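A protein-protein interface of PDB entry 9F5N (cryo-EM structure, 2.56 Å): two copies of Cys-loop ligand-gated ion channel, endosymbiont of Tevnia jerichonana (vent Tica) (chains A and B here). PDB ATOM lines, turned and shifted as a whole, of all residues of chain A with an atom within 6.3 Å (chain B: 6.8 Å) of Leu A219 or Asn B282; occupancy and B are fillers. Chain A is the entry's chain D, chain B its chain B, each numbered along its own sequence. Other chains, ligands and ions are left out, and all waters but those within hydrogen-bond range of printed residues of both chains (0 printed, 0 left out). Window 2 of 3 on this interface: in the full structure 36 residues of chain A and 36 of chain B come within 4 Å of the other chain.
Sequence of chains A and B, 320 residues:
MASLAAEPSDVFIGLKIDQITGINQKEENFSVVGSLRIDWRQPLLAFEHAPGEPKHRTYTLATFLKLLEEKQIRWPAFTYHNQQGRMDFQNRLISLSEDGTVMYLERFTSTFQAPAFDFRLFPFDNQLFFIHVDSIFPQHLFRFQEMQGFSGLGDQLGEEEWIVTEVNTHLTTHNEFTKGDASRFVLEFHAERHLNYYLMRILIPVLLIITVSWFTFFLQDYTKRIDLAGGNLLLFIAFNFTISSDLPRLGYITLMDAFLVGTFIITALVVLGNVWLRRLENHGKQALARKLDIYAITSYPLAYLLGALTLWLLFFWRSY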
ATOM      1  N   PHE A 215      15.078  13.923 -11.940  1.00  0.00           N
ATOM      2  CA  PHE A 215      15.441  12.526 -12.134  1.00  0.00           C
ATOM      3  C   PHE A 215      15.922  11.906 -10.830  1.00  0.00           C
ATOM      4  O   PHE A 215      15.525  10.789 -10.485  1.00  0.00           O
ATOM      5  CB  PHE A 215      16.507  12.397 -13.220  1.00  0.00           C
ATOM      6  N   THR A 216      16.749  12.629 -10.071  1.00  0.00           N
ATOM      7  CA  THR A 216      17.186  12.113  -8.779  1.00  0.00           C
ATOM      8  C   THR A 216      16.045  12.017  -7.774  1.00  0.00           C
ATOM      9  O   THR A 216      16.210  11.377  -6.733  1.00  0.00           O
ATOM     10  CB  THR A 216      18.304  12.986  -8.202  1.00  0.00           C
ATOM     11  N   PHE A 217      14.906  12.656  -8.045  1.00  0.00           N
ATOM     12  CA  PHE A 217      13.754  12.520  -7.159  1.00  0.00           C
ATOM     13  C   PHE A 217      13.150  11.121  -7.187  1.00  0.00           C
ATOM     14  O   PHE A 217      12.343  10.794  -6.311  1.00  0.00           O
ATOM     15  CB  PHE A 217      12.679  13.549  -7.516  1.00  0.00           C
ATOM     16  N   PHE A 218      13.481  10.303  -8.187  1.00  0.00           N
ATOM     17  CA  PHE A 218      12.958   8.941  -8.260  1.00  0.00           C
ATOM     18  C   PHE A 218      13.678   7.968  -7.333  1.00  0.00           C
ATOM     19  O   PHE A 218      13.405   6.765  -7.397  1.00  0.00           O
ATOM     20  CB  PHE A 218      13.035   8.429  -9.696  1.00  0.00           C
ATOM     21  N   LEU A 219      14.615   8.441  -6.512  1.00  0.00           N
ATOM     22  CA  LEU A 219      15.253   7.564  -5.537  1.00  0.00           C
ATOM     23  C   LEU A 219      14.258   7.088  -4.492  1.00  0.00           C
ATOM     24  O   LEU A 219      14.271   5.914  -4.102  1.00  0.00           O
ATOM     25  CB  LEU A 219      16.419   8.282  -4.862  1.00  0.00           C
ATOM     26  CG  LEU A 219      17.676   8.563  -5.677  1.00  0.00           C
ATOM     27  CD1 LEU A 219      18.702   9.239  -4.796  1.00  0.00           C
ATOM     28  CD2 LEU A 219      18.236   7.283  -6.267  1.00  0.00           C
ATOM     29  N   GLN A 220      13.373   7.980  -4.048  1.00  0.00           N
ATOM     30  CA  GLN A 220      12.469   7.727  -2.931  1.00  0.00           C
ATOM     31  C   GLN A 220      13.159   7.870  -1.579  1.00  0.00           C
ATOM     32  O   GLN A 220      12.779   7.199  -0.613  1.00  0.00           O
ATOM     33  CB  GLN A 220      11.840   6.340  -3.054  1.00  0.00           C
ATOM     34  N   ASP A 221      14.181   8.719  -1.500  1.00  0.00           N
ATOM     35  CA  ASP A 221      14.874   9.028  -0.245  1.00  0.00           C
ATOM     36  C   ASP A 221      14.723  10.521   0.068  1.00  0.00           C
ATOM     37  O   ASP A 221      15.520  11.343  -0.384  1.00  0.00           O
ATOM     38  CB  ASP A 221      16.338   8.631  -0.335  1.00  0.00           C
ATOM     39  CG  ASP A 221      17.143   9.133   0.836  1.00  0.00           C
ATOM     40  OD1 ASP A 221      16.616   9.122   1.968  1.00  0.00           O
ATOM     41  OD2 ASP A 221      18.293   9.568   0.619  1.00  0.00           O
ATOM     42  N   LYS A 224      17.636  12.858   0.738  1.00  0.00           N
ATOM     43  CA  LYS A 224      18.421  13.197  -0.440  1.00  0.00           C
ATOM     44  C   LYS A 224      17.770  14.331  -1.213  1.00  0.00           C
ATOM     45  O   LYS A 224      18.457  15.229  -1.713  1.00  0.00           O
ATOM     46  CB  LYS A 224      18.587  11.973  -1.337  1.00  0.00           C
ATOM     47  N   ARG A 225      16.443  14.308  -1.319  1.00  0.00           N
ATOM     48  CA  ARG A 225      15.742  15.400  -1.976  1.00  0.00           C
ATOM     49  C   ARG A 225      16.028  16.717  -1.281  1.00  0.00           C
ATOM     50  O   ARG A 225      16.324  17.722  -1.936  1.00  0.00           O
ATOM     51  CB  ARG A 225      14.243  15.123  -2.005  1.00  0.00           C
ATOM     52  CG  ARG A 225      13.868  13.925  -2.831  1.00  0.00           C
ATOM     53  CD  ARG A 225      12.379  13.668  -2.752  1.00  0.00           C
ATOM     54  NE  ARG A 225      11.995  12.522  -3.558  1.00  0.00           N
ATOM     55  CZ  ARG A 225      10.754  12.078  -3.679  1.00  0.00           C
ATOM     56  NH1 ARG A 225       9.750  12.652  -3.035  1.00  0.00           N
ATOM     57  NH2 ARG A 225      10.515  11.029  -4.462  1.00  0.00           N
ATOM     58  N   THR B 223      24.526   5.327  -5.033  1.00  0.00           N
ATOM     59  CA  THR B 223      24.347   6.653  -4.449  1.00  0.00           C
ATOM     60  C   THR B 223      25.619   7.485  -4.567  1.00  0.00           C
ATOM     61  O   THR B 223      25.562   8.697  -4.816  1.00  0.00           O
ATOM     62  CB  THR B 223      23.904   6.541  -2.993  1.00  0.00           C
ATOM     63  OG1 THR B 223      22.690   5.786  -2.916  1.00  0.00           O
ATOM     64  CG2 THR B 223      23.674   7.925  -2.406  1.00  0.00           C
ATOM     65  N   ILE B 226      25.762   8.920  -7.965  1.00  0.00           N
ATOM     66  CA  ILE B 226      24.871  10.057  -8.181  1.00  0.00           C
ATOM     67  C   ILE B 226      25.444  11.317  -7.544  1.00  0.00           C
ATOM     68  O   ILE B 226      25.474  12.390  -8.160  1.00  0.00           O
ATOM     69  CB  ILE B 226      23.459   9.746  -7.661  1.00  0.00           C
ATOM     70  CG1 ILE B 226      22.849   8.609  -8.472  1.00  0.00           C
ATOM     71  CG2 ILE B 226      22.599  10.985  -7.721  1.00  0.00           C
ATOM     72  CD1 ILE B 226      21.631   7.987  -7.836  1.00  0.00           C
ATOM     73  N   ASP B 227      25.905  11.208  -6.298  1.00  0.00           N
ATOM     74  CA  ASP B 227      26.499  12.361  -5.631  1.00  0.00           C
ATOM     75  C   ASP B 227      27.669  12.911  -6.436  1.00  0.00           C
ATOM     76  O   ASP B 227      27.721  14.111  -6.751  1.00  0.00           O
ATOM     77  CB  ASP B 227      26.955  11.968  -4.227  1.00  0.00           C
ATOM     78  CG  ASP B 227      25.817  11.497  -3.361  1.00  0.00           C
ATOM     79  OD1 ASP B 227      24.657  11.754  -3.737  1.00  0.00           O
ATOM     80  OD2 ASP B 227      26.073  10.876  -2.306  1.00  0.00           O
ATOM     81  N   ASN B 274      22.278   5.888 -13.028  1.00  0.00           N
ATOM     82  CA  ASN B 274      22.500   5.466 -11.648  1.00  0.00           C
ATOM     83  C   ASN B 274      21.204   5.436 -10.853  1.00  0.00           C
ATOM     84  O   ASN B 274      21.024   4.571  -9.994  1.00  0.00           O
ATOM     85  CB  ASN B 274      23.518   6.373 -10.965  1.00  0.00           C
ATOM     86  CG  ASN B 274      24.886   6.258 -11.578  1.00  0.00           C
ATOM     87  OD1 ASN B 274      25.671   7.202 -11.559  1.00  0.00           O
ATOM     88  ND2 ASN B 274      25.179   5.098 -12.144  1.00  0.00           N
ATOM     89  N   VAL B 275      20.302   6.383 -11.095  1.00  0.00           N
ATOM     90  CA  VAL B 275      19.010   6.339 -10.417  1.00  0.00           C
ATOM     91  C   VAL B 275      18.235   5.099 -10.838  1.00  0.00           C
ATOM     92  O   VAL B 275      17.597   4.436 -10.014  1.00  0.00           O
ATOM     93  CB  VAL B 275      18.205   7.621 -10.675  1.00  0.00           C
ATOM     94  CG1 VAL B 275      16.748   7.366 -10.379  1.00  0.00           C
ATOM     95  CG2 VAL B 275      18.709   8.736  -9.783  1.00  0.00           C
ATOM     96  N   TRP B 276      18.262   4.780 -12.132  1.00  0.00           N
ATOM     97  CA  TRP B 276      17.604   3.558 -12.586  1.00  0.00           C
ATOM     98  C   TRP B 276      18.214   2.328 -11.926  1.00  0.00           C
ATOM     99  O   TRP B 276      17.492   1.425 -11.494  1.00  0.00           O
ATOM    100  CB  TRP B 276      17.679   3.443 -14.106  1.00  0.00           C
ATOM    101  N   LEU B 277      19.543   2.273 -11.833  1.00  0.00           N
ATOM    102  CA  LEU B 277      20.183   1.147 -11.157  1.00  0.00           C
ATOM    103  C   LEU B 277      19.792   1.089  -9.683  1.00  0.00           C
ATOM    104  O   LEU B 277      19.586   0.004  -9.128  1.00  0.00           O
ATOM    105  CB  LEU B 277      21.702   1.238 -11.289  1.00  0.00           C
ATOM    106  CG  LEU B 277      22.365   1.055 -12.654  1.00  0.00           C
ATOM    107  CD1 LEU B 277      23.866   0.886 -12.463  1.00  0.00           C
ATOM    108  CD2 LEU B 277      21.781  -0.128 -13.414  1.00  0.00           C
ATOM    109  N   ARG B 278      19.701   2.249  -9.029  1.00  0.00           N
ATOM    110  CA  ARG B 278      19.412   2.278  -7.600  1.00  0.00           C
ATOM    111  C   ARG B 278      17.977   1.862  -7.312  1.00  0.00           C
ATOM    112  O   ARG B 278      17.705   1.232  -6.286  1.00  0.00           O
ATOM    113  CB  ARG B 278      19.687   3.668  -7.030  1.00  0.00           C
ATOM    114  CG  ARG B 278      19.524   3.762  -5.526  1.00  0.00           C
ATOM    115  CD  ARG B 278      20.461   2.804  -4.818  1.00  0.00           C
ATOM    116  NE  ARG B 278      20.658   3.138  -3.413  1.00  0.00           N
ATOM    117  CZ  ARG B 278      19.919   2.665  -2.421  1.00  0.00           C
ATOM    118  NH1 ARG B 278      18.906   1.846  -2.643  1.00  0.00           N
ATOM    119  NH2 ARG B 278      20.197   3.033  -1.172  1.00  0.00           N
ATOM    120  N   ARG B 279      17.041   2.214  -8.190  1.00  0.00           N
ATOM    121  CA  ARG B 279      15.680   1.712  -8.020  1.00  0.00           C
ATOM    122  C   ARG B 279      15.568   0.245  -8.427  1.00  0.00           C
ATOM    123  O   ARG B 279      14.726  -0.480  -7.888  1.00  0.00           O
ATOM    124  CB  ARG B 279      14.687   2.566  -8.810  1.00  0.00           C
ATOM    125  N   LEU B 280      16.395  -0.213  -9.369  1.00  0.00           N
ATOM    126  CA  LEU B 280      16.423  -1.638  -9.681  1.00  0.00           C
ATOM    127  C   LEU B 280      16.866  -2.442  -8.466  1.00  0.00           C
ATOM    128  O   LEU B 280      16.264  -3.466  -8.127  1.00  0.00           O
ATOM    129  CB  LEU B 280      17.344  -1.898 -10.876  1.00  0.00           C
ATOM    130  N   GLU B 281      17.919  -1.980  -7.790  1.00  0.00           N
ATOM    131  CA  GLU B 281      18.344  -2.605  -6.544  1.00  0.00           C
ATOM    132  C   GLU B 281      17.345  -2.369  -5.421  1.00  0.00           C
ATOM    133  O   GLU B 281      17.301  -3.155  -4.470  1.00  0.00           O
ATOM    134  CB  GLU B 281      19.725  -2.080  -6.131  1.00  0.00           C
ATOM    135  N   ASN B 282      16.549  -1.304  -5.508  1.00  0.00           N
ATOM    136  CA  ASN B 282      15.580  -1.008  -4.461  1.00  0.00           C
ATOM    137  C   ASN B 282      14.392  -1.966  -4.501  1.00  0.00           C
ATOM    138  O   ASN B 282      13.965  -2.475  -3.459  1.00  0.00           O
ATOM    139  CB  ASN B 282      15.115   0.440  -4.591  1.00  0.00           C
ATOM    140  CG  ASN B 282      14.257   0.874  -3.437  1.00  0.00           C
ATOM    141  OD1 ASN B 282      13.922   0.073  -2.566  1.00  0.00           O
ATOM    142  ND2 ASN B 282      13.891   2.149  -3.417  1.00  0.00           N
ATOM    143  N   HIS B 283      13.848  -2.232  -5.689  1.00  0.00           N
ATOM    144  CA  HIS B 283      12.666  -3.073  -5.833  1.00  0.00           C
ATOM    145  C   HIS B 283      13.010  -4.538  -6.077  1.00  0.00           C
ATOM    146  O   HIS B 283      12.233  -5.257  -6.720  1.00  0.00           O
ATOM    147  CB  HIS B 283      11.772  -2.541  -6.953  1.00  0.00           C
ATOM    148  CG  HIS B 283      11.168  -1.203  -6.659  1.00  0.00           C
ATOM    149  ND1 HIS B 283      10.766  -0.829  -5.395  1.00  0.00           N
ATOM    150  CD2 HIS B 283      10.897  -0.150  -7.465  1.00  0.00           C
ATOM    151  CE1 HIS B 283      10.274   0.395  -5.435  1.00  0.00           C
ATOM    152  NE2 HIS B 283      10.343   0.831  -6.680  1.00  0.00           N
ATOM    153  N   GLY B 284      14.154  -5.002  -5.581  1.00  0.00           N
ATOM    154  CA  GLY B 284      14.468  -6.410  -5.537  1.00  0.00           C
ATOM    155  C   GLY B 284      15.446  -6.893  -6.586  1.00  0.00           C
ATOM    156  O   GLY B 284      16.024  -7.973  -6.413  1.00  0.00           O
ATOM    157  N   LYS B 285      15.660  -6.128  -7.656  1.00  0.00           N
ATOM    158  CA  LYS B 285      16.517  -6.570  -8.757  1.00  0.00           C
ATOM    159  C   LYS B 285      17.954  -6.108  -8.514  1.00  0.00           C
ATOM    160  O   LYS B 285      18.495  -5.241  -9.198  1.00  0.00           O
ATOM    161  CB  LYS B 285      15.980  -6.058 -10.085  1.00  0.00           C
ATOM    162  N   GLN B 286      18.571  -6.709  -7.496  1.00  0.00           N
ATOM    163  CA  GLN B 286      19.976  -6.431  -7.216  1.00  0.00           C
ATOM    164  C   GLN B 286      20.900  -7.122  -8.218  1.00  0.00           C
ATOM    165  O   GLN B 286      21.889  -6.527  -8.662  1.00  0.00           O
ATOM    166  CB  GLN B 286      20.316  -6.857  -5.789  1.00  0.00           C
ATOM    167  N   ALA B 289      20.533  -5.486 -11.435  1.00  0.00           N
ATOM    168  CA  ALA B 289      21.190  -4.197 -11.278  1.00  0.00           C
ATOM    169  C   ALA B 289      22.690  -4.319 -11.503  1.00  0.00           C
ATOM    170  O   ALA B 289      23.281  -3.516 -12.228  1.00  0.00           O
ATOM    171  CB  ALA B 289      20.885  -3.620  -9.895  1.00  0.00           C
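Along chain A the printed residues that touch a printed residue of chain B span positions 215 to 219. Printed residues of chain B that touch a printed residue of chain A: Ile B226, Val B275, Arg B278 and Asn B282. Hydrophobic or aromatic side chains of chain B that line the printed part of chain A: Ile B226 and Val B275. Among the printed residues, no Asp or Glu carboxylate lies within 4 Å of a Lys or Arg side-chain nitrogen of the other chain.
Of chain B, only Ile B226, Val B275, Arg B278 and Asn B282 come within 4 Å of Leu A219. Asn B282 touches just one residue of chain A: Leu A219. Printed residues of chain A within 4 Å of Val B275: Phe A215, Thr A216, Phe A218 and Leu A219. Printed residues of chain A within 4 Å of Ile B226: Leu A219 (3.8 Å). Of the printed residues of chain B, Thr A216 touches Val B275 (3.8 Å). Printed residues of chain B within 4 Å of Phe A215: Val B275 (3.6 Å). Printed residues of chain A within 4 Å of Arg B278: Leu A219. Gln A220 touches none of the printed residues of chain B. Glu B281 touches none of the printed residues of chain A. The nearest residue of chain A that does not touch Asn B282 is Gln A220 (4.7 Å).
CG1 of Val B275 touches O of Phe A215, 3.6 Å away. Thr A216 touches Val B275 (CA to CG2, 3.8 Å). Phe A218 touches Val B275 (CB to CG1, 3.9 Å). Ile B226 touches Leu A219 (CD1 to CD2, 3.8 Å). CG2 of Val B275 touches CD2 of Leu A219 (3.8 Å). Leu A219 touches Arg B278. Leu A219 touches Asn B282.
OG1 of Thr B223 is in hydrogen-bond range of NE of Arg B278 (3.4 Å).
No position is printed for both chains.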
